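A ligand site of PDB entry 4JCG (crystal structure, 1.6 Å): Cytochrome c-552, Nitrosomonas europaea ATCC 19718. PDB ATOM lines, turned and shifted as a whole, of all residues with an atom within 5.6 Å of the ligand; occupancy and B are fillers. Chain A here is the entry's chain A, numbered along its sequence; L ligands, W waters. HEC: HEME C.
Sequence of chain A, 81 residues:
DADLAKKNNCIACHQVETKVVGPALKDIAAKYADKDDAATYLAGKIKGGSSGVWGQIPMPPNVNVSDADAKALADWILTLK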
ATOM      1  N   ALA A   5       1.543  -6.416 -29.996  1.00  0.00           N
ATOM      2  CA  ALA A   5       2.198  -5.257 -29.411  1.00  0.00           C
ATOM      3  C   ALA A   5       3.397  -5.768 -28.616  1.00  0.00           C
ATOM      4  O   ALA A   5       4.457  -5.167 -28.634  1.00  0.00           O
ATOM      5  CB  ALA A   5       1.246  -4.479 -28.518  1.00  0.00           C
ATOM      6  N   ASN A   8       6.238  -6.960 -31.077  1.00  0.00           N
ATOM      7  CA  ASN A   8       6.949  -5.821 -31.651  1.00  0.00           C
ATOM      8  C   ASN A   8       7.518  -4.820 -30.669  1.00  0.00           C
ATOM      9  O   ASN A   8       7.848  -3.678 -31.049  1.00  0.00           O
ATOM     10  CB  ASN A   8       6.038  -5.098 -32.649  1.00  0.00           C
ATOM     11  CG  ASN A   8       5.827  -5.931 -33.887  1.00  0.00           C
ATOM     12  OD1 ASN A   8       6.628  -5.871 -34.809  1.00  0.00           O
ATOM     13  ND2 ASN A   8       4.769  -6.740 -33.889  1.00  0.00           N
ATOM     14  N   ASN A   9       7.562  -5.230 -29.394  1.00  0.00           N
ATOM     15  CA  ASN A   9       8.257  -4.520 -28.332  1.00  0.00           C
ATOM     16  C   ASN A   9       7.632  -3.171 -28.037  1.00  0.00           C
ATOM     17  O   ASN A   9       8.332  -2.229 -27.642  1.00  0.00           O
ATOM     18  CB  ASN A   9       9.737  -4.361 -28.673  1.00  0.00           C
ATOM     19  CG  ASN A   9      10.587  -3.969 -27.472  1.00  0.00           C
ATOM     20  OD1 ASN A   9      10.216  -4.213 -26.315  1.00  0.00           O
ATOM     21  ND2 ASN A   9      11.715  -3.329 -27.751  1.00  0.00           N
ATOM     22  N   CYS A  10       6.328  -3.073 -28.204  1.00  0.00           N
ATOM     23  CA  CYS A  10       5.661  -1.826 -27.886  1.00  0.00           C
ATOM     24  C   CYS A  10       5.393  -1.693 -26.404  1.00  0.00           C
ATOM     25  O   CYS A  10       5.200  -0.575 -25.907  1.00  0.00           O
ATOM     26  CB  CYS A  10       4.343  -1.663 -28.626  1.00  0.00           C
ATOM     27  SG  CYS A  10       4.501  -2.149 -30.309  1.00  0.00           S
ATOM     28  N   ALA A  12       7.186  -2.130 -23.756  1.00  0.00           N
ATOM     29  CA  ALA A  12       8.210  -1.532 -22.903  1.00  0.00           C
ATOM     30  C   ALA A  12       7.743  -0.130 -22.558  1.00  0.00           C
ATOM     31  O   ALA A  12       7.942   0.364 -21.436  1.00  0.00           O
ATOM     32  CB  ALA A  12       9.526  -1.458 -23.668  1.00  0.00           C
ATOM     33  N   CYS A  13       7.094   0.499 -23.526  1.00  0.00           N
ATOM     34  CA  CYS A  13       6.770   1.913 -23.405  1.00  0.00           C
ATOM     35  C   CYS A  13       5.281   2.246 -23.325  1.00  0.00           C
ATOM     36  O   CYS A  13       4.958   3.360 -22.950  1.00  0.00           O
ATOM     37  CB  CYS A  13       7.419   2.684 -24.552  1.00  0.00           C
ATOM     38  SG  CYS A  13       9.252   2.615 -24.638  1.00  0.00           S
ATOM     39  N   HIS A  14       4.385   1.332 -23.638  1.00  0.00           N
ATOM     40  CA  HIS A  14       2.969   1.675 -23.698  1.00  0.00           C
ATOM     41  C   HIS A  14       2.106   0.601 -23.031  1.00  0.00           C
ATOM     42  O   HIS A  14       2.294  -0.567 -23.303  1.00  0.00           O
ATOM     43  CB  HIS A  14       2.462   1.764 -25.165  1.00  0.00           C
ATOM     44  CG  HIS A  14       3.058   2.865 -25.995  1.00  0.00           C
ATOM     45  ND1 HIS A  14       2.580   4.163 -25.986  1.00  0.00           N
ATOM     46  CD2 HIS A  14       4.015   2.839 -26.965  1.00  0.00           C
ATOM     47  CE1 HIS A  14       3.238   4.884 -26.860  1.00  0.00           C
ATOM     48  NE2 HIS A  14       4.117   4.112 -27.467  1.00  0.00           N
ATOM     49  N   VAL A  21       5.784   5.228 -20.569  1.00  0.00           N
ATOM     50  CA  VAL A  21       6.741   6.141 -21.219  1.00  0.00           C
ATOM     51  C   VAL A  21       6.057   6.946 -22.320  1.00  0.00           C
ATOM     52  O   VAL A  21       6.069   8.173 -22.320  1.00  0.00           O
ATOM     53  CB  VAL A  21       7.911   5.384 -21.828  1.00  0.00           C
ATOM     54  CG1 VAL A  21       8.823   6.325 -22.630  1.00  0.00           C
ATOM     55  CG2 VAL A  21       8.680   4.619 -20.717  1.00  0.00           C
ATOM     56  N   GLY A  22       5.455   6.264 -23.276  1.00  0.00           N
ATOM     57  CA  GLY A  22       4.648   6.982 -24.239  1.00  0.00           C
ATOM     58  C   GLY A  22       3.260   6.955 -23.676  1.00  0.00           C
ATOM     59  O   GLY A  22       3.024   6.386 -22.627  1.00  0.00           O
ATOM     60  N   PRO A  23       2.321   7.576 -24.388  1.00  0.00           N
ATOM     61  CA  PRO A  23       0.933   7.667 -23.957  1.00  0.00           C
ATOM     62  C   PRO A  23       0.212   6.299 -23.830  1.00  0.00           C
ATOM     63  O   PRO A  23       0.510   5.331 -24.559  1.00  0.00           O
ATOM     64  CB  PRO A  23       0.311   8.529 -25.056  1.00  0.00           C
ATOM     65  CG  PRO A  23       1.228   8.328 -26.285  1.00  0.00           C
ATOM     66  CD  PRO A  23       2.580   8.278 -25.664  1.00  0.00           C
ATOM     67  N   LEU A  25      -2.415   3.637 -24.590  1.00  0.00           N
ATOM     68  CA  LEU A  25      -2.961   3.382 -25.909  1.00  0.00           C
ATOM     69  C   LEU A  25      -4.403   3.848 -26.009  1.00  0.00           C
ATOM     70  O   LEU A  25      -4.797   4.354 -27.045  1.00  0.00           O
ATOM     71  CB  LEU A  25      -2.828   1.891 -26.298  1.00  0.00           C
ATOM     72  CG  LEU A  25      -1.373   1.427 -26.297  1.00  0.00           C
ATOM     73  CD1 LEU A  25      -1.267  -0.054 -26.671  1.00  0.00           C
ATOM     74  CD2 LEU A  25      -0.511   2.233 -27.248  1.00  0.00           C
ATOM     75  N   ILE A  28      -4.443   7.412 -26.917  1.00  0.00           N
ATOM     76  CA  ILE A  28      -4.259   7.571 -28.331  1.00  0.00           C
ATOM     77  C   ILE A  28      -5.576   7.325 -29.079  1.00  0.00           C
ATOM     78  O   ILE A  28      -5.898   8.097 -29.980  1.00  0.00           O
ATOM     79  CB  ILE A  28      -3.147   6.624 -28.840  1.00  0.00           C
ATOM     80  CG1 ILE A  28      -1.817   6.958 -28.178  1.00  0.00           C
ATOM     81  CG2 ILE A  28      -3.007   6.701 -30.342  1.00  0.00           C
ATOM     82  CD1 ILE A  28      -0.743   5.883 -28.480  1.00  0.00           C
ATOM     83  N   LYS A  31      -7.868  10.396 -28.727  1.00  0.00           N
ATOM     84  CA  LYS A  31      -7.431  11.582 -29.413  1.00  0.00           C
ATOM     85  C   LYS A  31      -7.800  11.559 -30.884  1.00  0.00           C
ATOM     86  O   LYS A  31      -8.128  12.597 -31.458  1.00  0.00           O
ATOM     87  CB  LYS A  31      -5.918  11.788 -29.243  1.00  0.00           C
ATOM     88  CG  LYS A  31      -5.359  12.991 -30.010  1.00  0.00           C
ATOM     89  CD  LYS A  31      -3.869  13.172 -29.743  1.00  0.00           C
ATOM     90  CE  LYS A  31      -3.347  14.412 -30.455  1.00  0.00           C
ATOM     91  NZ  LYS A  31      -3.909  15.553 -29.719  1.00  0.00           N
ATOM     92  N   TYR A  32      -7.699  10.372 -31.489  1.00  0.00           N
ATOM     93  CA  TYR A  32      -7.807  10.243 -32.938  1.00  0.00           C
ATOM     94  C   TYR A  32      -9.122   9.656 -33.434  1.00  0.00           C
ATOM     95  O   TYR A  32      -9.252   9.284 -34.592  1.00  0.00           O
ATOM     96  CB  TYR A  32      -6.645   9.434 -33.439  1.00  0.00           C
ATOM     97  CG  TYR A  32      -5.327  10.146 -33.204  1.00  0.00           C
ATOM     98  CD1 TYR A  32      -5.073  11.336 -33.838  1.00  0.00           C
ATOM     99  CD2 TYR A  32      -4.354   9.624 -32.363  1.00  0.00           C
ATOM    100  CE1 TYR A  32      -3.877  12.001 -33.633  1.00  0.00           C
ATOM    101  CE2 TYR A  32      -3.142  10.298 -32.174  1.00  0.00           C
ATOM    102  CZ  TYR A  32      -2.915  11.471 -32.829  1.00  0.00           C
ATOM    103  OH  TYR A  32      -1.759  12.204 -32.680  1.00  0.00           O
ATOM    104  N   TYR A  41      -2.330   7.237 -40.579  1.00  0.00           N
ATOM    105  CA  TYR A  41      -1.501   8.228 -39.881  1.00  0.00           C
ATOM    106  C   TYR A  41      -0.696   7.574 -38.740  1.00  0.00           C
ATOM    107  O   TYR A  41       0.504   7.759 -38.646  1.00  0.00           O
ATOM    108  CB  TYR A  41      -2.356   9.370 -39.327  1.00  0.00           C
ATOM    109  CG  TYR A  41      -1.643  10.240 -38.294  1.00  0.00           C
ATOM    110  CD1 TYR A  41      -0.746  11.237 -38.679  1.00  0.00           C
ATOM    111  CD2 TYR A  41      -1.863  10.037 -36.935  1.00  0.00           C
ATOM    112  CE1 TYR A  41      -0.077  12.016 -37.731  1.00  0.00           C
ATOM    113  CE2 TYR A  41      -1.208  10.797 -35.968  1.00  0.00           C
ATOM    114  CZ  TYR A  41      -0.326  11.790 -36.369  1.00  0.00           C
ATOM    115  OH  TYR A  41       0.320  12.509 -35.401  1.00  0.00           O
ATOM    116  N   LEU A  42      -1.384   6.813 -37.903  1.00  0.00           N
ATOM    117  CA  LEU A  42      -0.675   6.200 -36.765  1.00  0.00           C
ATOM    118  C   LEU A  42       0.304   5.135 -37.243  1.00  0.00           C
ATOM    119  O   LEU A  42       1.372   4.974 -36.644  1.00  0.00           O
ATOM    120  CB  LEU A  42      -1.674   5.527 -35.804  1.00  0.00           C
ATOM    121  CG  LEU A  42      -2.522   6.544 -34.992  1.00  0.00           C
ATOM    122  CD1 LEU A  42      -3.479   5.801 -34.039  1.00  0.00           C
ATOM    123  CD2 LEU A  42      -1.702   7.534 -34.185  1.00  0.00           C
ATOM    124  N   LYS A  45       3.383   6.941 -37.991  1.00  0.00           N
ATOM    125  CA  LYS A  45       4.117   7.287 -36.767  1.00  0.00           C
ATOM    126  C   LYS A  45       4.827   6.086 -36.152  1.00  0.00           C
ATOM    127  O   LYS A  45       5.949   6.196 -35.658  1.00  0.00           O
ATOM    128  CB  LYS A  45       3.158   7.927 -35.737  1.00  0.00           C
ATOM    129  CG  LYS A  45       2.518   9.229 -36.171  1.00  0.00           C
ATOM    130  CD  LYS A  45       3.660  10.193 -36.576  1.00  0.00           C
ATOM    131  CE  LYS A  45       3.343  11.626 -36.356  1.00  0.00           C
ATOM    132  NZ  LYS A  45       3.289  12.074 -34.928  1.00  0.00           N
ATOM    133  N   ILE A  46       4.211   4.913 -36.182  1.00  0.00           N
ATOM    134  CA  ILE A  46       4.853   3.721 -35.655  1.00  0.00           C
ATOM    135  C   ILE A  46       6.123   3.392 -36.480  1.00  0.00           C
ATOM    136  O   ILE A  46       7.195   3.102 -35.918  1.00  0.00           O
ATOM    137  CB  ILE A  46       3.864   2.526 -35.679  1.00  0.00           C
ATOM    138  CG1 ILE A  46       2.768   2.781 -34.623  1.00  0.00           C
ATOM    139  CG2 ILE A  46       4.590   1.209 -35.416  1.00  0.00           C
ATOM    140  CD1 ILE A  46       1.480   1.934 -34.880  1.00  0.00           C
ATOM    141  N   SER A  50       7.913   9.451 -33.719  1.00  0.00           N
ATOM    142  CA  SER A  50       7.064  10.588 -33.357  1.00  0.00           C
ATOM    143  C   SER A  50       7.750  11.473 -32.341  1.00  0.00           C
ATOM    144  O   SER A  50       8.457  10.999 -31.444  1.00  0.00           O
ATOM    145  CB  SER A  50       5.736  10.088 -32.785  1.00  0.00           C
ATOM    146  OG  SER A  50       4.791  11.160 -32.615  1.00  0.00           O
ATOM    147  N   SER A  51       7.520  12.771 -32.445  1.00  0.00           N
ATOM    148  CA  SER A  51       7.896  13.653 -31.350  1.00  0.00           C
ATOM    149  C   SER A  51       7.025  14.907 -31.336  1.00  0.00           C
ATOM    150  O   SER A  51       6.491  15.341 -32.358  1.00  0.00           O
ATOM    151  CB  SER A  51       9.376  14.012 -31.384  1.00  0.00           C
ATOM    152  OG  SER A  51       9.715  14.807 -30.248  1.00  0.00           O
ATOM    153  N   GLY A  52       6.849  15.443 -30.136  1.00  0.00           N
ATOM    154  CA  GLY A  52       6.081  16.656 -29.951  1.00  0.00           C
ATOM    155  C   GLY A  52       4.562  16.525 -29.775  1.00  0.00           C
ATOM    156  O   GLY A  52       3.930  17.520 -29.402  1.00  0.00           O
ATOM    157  N   VAL A  53       3.992  15.360 -30.106  1.00  0.00           N
ATOM    158  CA  VAL A  53       2.558  15.220 -29.963  1.00  0.00           C
ATOM    159  C   VAL A  53       2.138  15.090 -28.498  1.00  0.00           C
ATOM    160  O   VAL A  53       1.084  15.616 -28.085  1.00  0.00           O
ATOM    161  CB  VAL A  53       2.054  14.075 -30.816  1.00  0.00           C
ATOM    162  CG1 VAL A  53       0.550  13.980 -30.726  1.00  0.00           C
ATOM    163  CG2 VAL A  53       2.489  14.349 -32.284  1.00  0.00           C
ATOM    164  N   TRP A  54       2.943  14.389 -27.719  1.00  0.00           N
ATOM    165  CA  TRP A  54       2.603  14.070 -26.321  1.00  0.00           C
ATOM    166  C   TRP A  54       3.614  14.651 -25.333  1.00  0.00           C
ATOM    167  O   TRP A  54       3.374  14.611 -24.130  1.00  0.00           O
ATOM    168  CB  TRP A  54       2.519  12.534 -26.140  1.00  0.00           C
ATOM    169  CG  TRP A  54       1.487  11.912 -27.060  1.00  0.00           C
ATOM    170  CD1 TRP A  54       1.681  11.459 -28.367  1.00  0.00           C
ATOM    171  CD2 TRP A  54       0.098  11.690 -26.773  1.00  0.00           C
ATOM    172  NE1 TRP A  54       0.487  10.974 -28.867  1.00  0.00           N
ATOM    173  CE2 TRP A  54      -0.487  11.110 -27.905  1.00  0.00           C
ATOM    174  CE3 TRP A  54      -0.696  11.923 -25.651  1.00  0.00           C
ATOM    175  CZ2 TRP A  54      -1.829  10.775 -27.969  1.00  0.00           C
ATOM    176  CZ3 TRP A  54      -2.045  11.590 -25.702  1.00  0.00           C
ATOM    177  CH2 TRP A  54      -2.604  11.018 -26.854  1.00  0.00           C
ATOM    178  N   GLY A  55       4.754  15.127 -25.836  1.00  0.00           N
ATOM    179  CA  GLY A  55       5.835  15.588 -24.980  1.00  0.00           C
ATOM    180  C   GLY A  55       7.041  15.753 -25.861  1.00  0.00           C
ATOM    181  O   GLY A  55       6.924  15.708 -27.081  1.00  0.00           O
ATOM    182  N   GLN A  56       8.201  15.990 -25.256  1.00  0.00           N
ATOM    183  CA  GLN A  56       9.414  16.226 -26.037  1.00  0.00           C
ATOM    184  C   GLN A  56      10.343  15.023 -26.025  1.00  0.00           C
ATOM    185  O   GLN A  56      11.515  15.136 -26.354  1.00  0.00           O
ATOM    186  CB  GLN A  56      10.140  17.445 -25.485  1.00  0.00           C
ATOM    187  CG  GLN A  56       9.255  18.748 -25.477  1.00  0.00           C
ATOM    188  CD  GLN A  56       8.766  19.103 -26.889  1.00  0.00           C
ATOM    189  OE1 GLN A  56       9.575  19.215 -27.814  1.00  0.00           O
ATOM    190  NE2 GLN A  56       7.441  19.283 -27.047  1.00  0.00           N
ATOM    191  N   ILE A  57       9.810  13.894 -25.589  1.00  0.00           N
ATOM    192  CA  ILE A  57      10.571  12.637 -25.624  1.00  0.00           C
ATOM    193  C   ILE A  57      10.157  11.875 -26.872  1.00  0.00           C
ATOM    194  O   ILE A  57       9.023  11.428 -26.983  1.00  0.00           O
ATOM    195  CB  ILE A  57      10.266  11.792 -24.380  1.00  0.00           C
ATOM    196  CG1 ILE A  57      10.770  12.471 -23.119  1.00  0.00           C
ATOM    197  CG2 ILE A  57      10.940  10.407 -24.511  1.00  0.00           C
ATOM    198  CD1 ILE A  57       9.999  12.032 -21.891  1.00  0.00           C
ATOM    199  N   PRO A  58      11.063  11.751 -27.849  1.00  0.00           N
ATOM    200  CA  PRO A  58      10.639  11.129 -29.113  1.00  0.00           C
ATOM    201  C   PRO A  58      10.501   9.625 -29.008  1.00  0.00           C
ATOM    202  O   PRO A  58      11.242   8.945 -28.300  1.00  0.00           O
ATOM    203  CB  PRO A  58      11.785  11.448 -30.073  1.00  0.00           C
ATOM    204  CG  PRO A  58      12.655  12.483 -29.375  1.00  0.00           C
ATOM    205  CD  PRO A  58      12.447  12.251 -27.906  1.00  0.00           C
ATOM    206  N   MET A  59       9.514   9.096 -29.727  1.00  0.00           N
ATOM    207  CA  MET A  59       9.494   7.676 -29.992  1.00  0.00           C
ATOM    208  C   MET A  59      10.431   7.417 -31.161  1.00  0.00           C
ATOM    209  O   MET A  59      10.250   7.973 -32.247  1.00  0.00           O
ATOM    210  CB  MET A  59       8.080   7.223 -30.382  1.00  0.00           C
ATOM    211  CG  MET A  59       8.068   5.792 -30.870  1.00  0.00           C
ATOM    212  SD  MET A  59       6.488   5.035 -31.222  1.00  0.00           S
ATOM    213  CE  MET A  59       5.685   6.254 -32.292  1.00  0.00           C
ATOM    214  N   PRO A  60      11.453   6.561 -30.974  1.00  0.00           N
ATOM    215  CA  PRO A  60      12.263   6.192 -32.126  1.00  0.00           C
ATOM    216  C   PRO A  60      11.458   5.433 -33.178  1.00  0.00           C
ATOM    217  O   PRO A  60      10.522   4.723 -32.822  1.00  0.00           O
ATOM    218  CB  PRO A  60      13.293   5.219 -31.534  1.00  0.00           C
ATOM    219  CG  PRO A  60      13.347   5.550 -30.070  1.00  0.00           C
ATOM    220  CD  PRO A  60      11.901   5.915 -29.733  1.00  0.00           C
ATOM    221  N   ASN A  62      10.318   2.476 -35.332  1.00  0.00           N
ATOM    222  CA  ASN A  62      10.270   1.061 -35.016  1.00  0.00           C
ATOM    223  C   ASN A  62      10.685   0.298 -36.279  1.00  0.00           C
ATOM    224  O   ASN A  62       9.839  -0.186 -37.048  1.00  0.00           O
ATOM    225  CB  ASN A  62       8.857   0.688 -34.542  1.00  0.00           C
ATOM    226  CG  ASN A  62       8.520   1.343 -33.237  1.00  0.00           C
ATOM    227  OD1 ASN A  62       9.049   0.953 -32.190  1.00  0.00           O
ATOM    228  ND2 ASN A  62       7.650   2.371 -33.281  1.00  0.00           N
ATOM    229  N   VAL A  65       9.383  -3.227 -37.522  1.00  0.00           N
ATOM    230  CA  VAL A  65       7.939  -3.482 -37.712  1.00  0.00           C
ATOM    231  C   VAL A  65       7.632  -3.475 -39.218  1.00  0.00           C
ATOM    232  O   VAL A  65       8.028  -2.553 -39.932  1.00  0.00           O
ATOM    233  CB  VAL A  65       7.081  -2.447 -36.964  1.00  0.00           C
ATOM    234  CG1 VAL A  65       5.609  -2.866 -36.984  1.00  0.00           C
ATOM    235  CG2 VAL A  65       7.547  -2.457 -35.556  1.00  0.00           C
ATOM    236  N   LEU A  73      -1.316  -2.838 -35.811  1.00  0.00           N
ATOM    237  CA  LEU A  73      -1.189  -2.159 -34.485  1.00  0.00           C
ATOM    238  C   LEU A  73      -1.967  -0.873 -34.398  1.00  0.00           C
ATOM    239  O   LEU A  73      -2.614  -0.637 -33.381  1.00  0.00           O
ATOM    240  CB  LEU A  73       0.265  -1.936 -34.089  1.00  0.00           C
ATOM    241  CG  LEU A  73       0.978  -3.258 -33.799  1.00  0.00           C
ATOM    242  CD1 LEU A  73       2.494  -3.021 -33.902  1.00  0.00           C
ATOM    243  CD2 LEU A  73       0.635  -3.750 -32.396  1.00  0.00           C
ATOM    244  N   ILE A  77      -5.023  -0.283 -31.778  1.00  0.00           N
ATOM    245  CA  ILE A  77      -5.043   0.892 -30.898  1.00  0.00           C
ATOM    246  C   ILE A  77      -6.332   1.711 -31.042  1.00  0.00           C
ATOM    247  O   ILE A  77      -6.938   2.111 -30.041  1.00  0.00           O
ATOM    248  CB  ILE A  77      -3.770   1.763 -31.151  1.00  0.00           C
ATOM    249  CG1 ILE A  77      -2.531   0.998 -30.642  1.00  0.00           C
ATOM    250  CG2 ILE A  77      -3.932   3.095 -30.454  1.00  0.00           C
ATOM    251  CD1 ILE A  77      -1.193   1.627 -31.022  1.00  0.00           C
HETATM  252 FE   HEC L   1       5.251   4.626 -29.230  1.00  0.00          FE
HETATM  253  CHA HEC L   1       3.930   7.760 -29.434  1.00  0.00           C
HETATM  254  CHB HEC L   1       2.649   3.358 -31.059  1.00  0.00           C
HETATM  255  CHC HEC L   1       6.760   1.517 -29.307  1.00  0.00           C
HETATM  256  CHD HEC L   1       7.446   5.577 -26.833  1.00  0.00           C
HETATM  257  NA  HEC L   1       3.610   5.380 -30.045  1.00  0.00           N
HETATM  258  C1A HEC L   1       3.273   6.729 -30.045  1.00  0.00           C
HETATM  259  C2A HEC L   1       2.068   6.863 -30.833  1.00  0.00           C
HETATM  260  C3A HEC L   1       1.717   5.667 -31.274  1.00  0.00           C
HETATM  261  C4A HEC L   1       2.680   4.738 -30.799  1.00  0.00           C
HETATM  262  CMA HEC L   1       0.494   5.304 -32.141  1.00  0.00           C
HETATM  263  CAA HEC L   1       1.331   8.212 -31.026  1.00  0.00           C
HETATM  264  CBA HEC L   1       1.860   9.042 -32.183  1.00  0.00           C
HETATM  265  CGA HEC L   1       0.939  10.224 -32.415  1.00  0.00           C
HETATM  266  O1A HEC L   1       0.017  10.594 -31.646  1.00  0.00           O
HETATM  267  O2A HEC L   1       1.183  10.935 -33.423  1.00  0.00           O
HETATM  268  NB  HEC L   1       4.826   2.846 -30.024  1.00  0.00           N
HETATM  269  C1B HEC L   1       3.698   2.509 -30.743  1.00  0.00           C
HETATM  270  C2B HEC L   1       3.821   1.171 -31.184  1.00  0.00           C
HETATM  271  C3B HEC L   1       4.924   0.637 -30.685  1.00  0.00           C
HETATM  272  C4B HEC L   1       5.593   1.674 -29.994  1.00  0.00           C
HETATM  273  CMB HEC L   1       2.702   0.434 -31.916  1.00  0.00           C
HETATM  274  CAB HEC L   1       5.468  -0.805 -30.948  1.00  0.00           C
HETATM  275  CBB HEC L   1       5.796  -0.960 -32.474  1.00  0.00           C
HETATM  276  NC  HEC L   1       6.704   3.718 -28.221  1.00  0.00           N
HETATM  277  C1C HEC L   1       7.261   2.468 -28.453  1.00  0.00           C
HETATM  278  C2C HEC L   1       8.532   2.346 -27.794  1.00  0.00           C
HETATM  279  C3C HEC L   1       8.702   3.440 -27.056  1.00  0.00           C
HETATM  280  C4C HEC L   1       7.595   4.328 -27.353  1.00  0.00           C
HETATM  281  CMC HEC L   1       9.315   1.025 -27.800  1.00  0.00           C
HETATM  282  CAC HEC L   1       9.817   3.761 -26.032  1.00  0.00           C
HETATM  283  CBC HEC L   1      11.235   3.571 -26.515  1.00  0.00           C
HETATM  284  ND  HEC L   1       5.578   6.332 -28.349  1.00  0.00           N
HETATM  285  C1D HEC L   1       6.603   6.520 -27.398  1.00  0.00           C
HETATM  286  C2D HEC L   1       6.645   7.911 -27.027  1.00  0.00           C
HETATM  287  C3D HEC L   1       5.569   8.588 -27.808  1.00  0.00           C
HETATM  288  C4D HEC L   1       4.975   7.560 -28.597  1.00  0.00           C
HETATM  289  CMD HEC L   1       7.605   8.561 -26.028  1.00  0.00           C
HETATM  290  CAD HEC L   1       5.182  10.073 -27.823  1.00  0.00           C
HETATM  291  CBD HEC L   1       5.824  10.707 -29.044  1.00  0.00           C
HETATM  292  CGD HEC L   1       5.396  12.126 -29.171  1.00  0.00           C
HETATM  293  O1D HEC L   1       5.079  12.558 -30.309  1.00  0.00           O
HETATM  294  O2D HEC L   1       5.325  12.883 -28.155  1.00  0.00           O
HETATM  295  O   HOH W   1      10.592   6.847 -26.063  1.00  0.00           O
HETATM  296  O   HOH W   2       6.868  12.495 -25.892  1.00  0.00           O
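O of Asn 8 touches CBB of the ligand (3.7 Å). Asn 9 touches the ligand. Gly 22 touches the ligand (CA to C2D, 3.6 Å). Pro 23 touches the ligand (CD to C3D, 3.7 Å). Ile 28 touches the ligand. Leu 42 touches the ligand. Ile 46 touches the ligand (CD1 to CMB, 3.5 Å). Ile 57 touches the ligand (O to CMD, 3.3 Å). CG of Asn 62 touches CBB of the ligand, 3.6 Å away. CG2 of Val 65 touches CBB of the ligand, 3.8 Å away. Leu 73 touches the ligand (CD1 to CMB, 3.99 Å). Hydrophobic or aromatic side chains that line the ligand: His 14, Pro 23, Ile 28, Tyr 32, Tyr 41, Leu 42, Ile 46, Val 53, Trp 54, Met 59, Val 65 and Leu 73. Of the 33 residues printed, 24 come within 4 Å of the ligand.
The backbone NH of Gly 22 lies within hydrogen-bond range of the backbone carbonyl oxygen of Cys 13, 3.0 Å away. The backbone NH of Val 21 lies within hydrogen-bond range of the backbone carbonyl oxygen of Cys 13 (3.1 Å). ND1 of His 14 lies within hydrogen-bond range of O of Pro 23, 2.8 Å away. The backbone NH (N) of Met 59 is in hydrogen-bond range of the backbone carbonyl oxygen (O) of Ser 50 (2.8 Å). SD of Met 59 lies close to ND2 of Asn 62 (3.6 Å). The side-chain hydroxyl of Tyr 41 lies within hydrogen-bond range of the side-chain amino group of Lys 45 (3.0 Å). The side-chain amino group (NZ) of Lys 45 sits at hydrogen-bond distance from the side-chain hydroxyl (OG) of Ser 50 (2.9 Å). O of Ile 46 is in hydrogen-bond range of ND2 of Asn 62.
Water W2 lies within hydrogen-bond range of the backbone carbonyl oxygen (O) of Ile 57 (2.6 Å), an oxygen (O2D) of the ligand (2.8 Å) and the backbone NH (N) of Gly 55 (3.4 Å).
The side-chain sulfur (SG) of Cys 10 is bonded to a carbon (CAB) of the ligand (1.8 Å). SG of Cys 13 is covalently linked to CAC of the ligand (1.9 Å). NE2 of His 14 is bound to FE of the ligand (2.2 Å). An iron atom (FE) of the ligand is bound by the side-chain sulfur of Met 59, 2.4 Å away. OH of Tyr 32 lies within hydrogen-bond range of O1A of the ligand, at 2.6 Å. The side-chain hydroxyl (OH) of Tyr 41 sits at hydrogen-bond distance from an oxygen (O2A) of the ligand (2.7 Å). The side-chain hydroxyl (OG) of Ser 50 lies within hydrogen-bond range of an oxygen (O1D) of the ligand (2.7 Å). The side-chain amino group (NZ) of Lys 45 is in salt-bridge range of an oxygen (O2A) of the ligand (2.8 Å). The backbone NH of Trp 54 lies within hydrogen-bond range of an oxygen (O2D) of the ligand, at 2.9 Å. An oxygen (O1A) of the ligand lies within hydrogen-bond range of the indole nitrogen of Trp 54. The backbone NH (N) of Val 53 sits at hydrogen-bond distance from an oxygen (O1D) of the ligand (3.0 Å). N of Ser 51 sits close to O1D of the ligand, 3.3 Å away. N of Gly 55 lies within hydrogen-bond range of O2D of the ligand (3.3 Å). The backbone NH (N) of Gly 52 is in hydrogen-bond range of an oxygen (O1D) of the ligand (3.4 Å).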
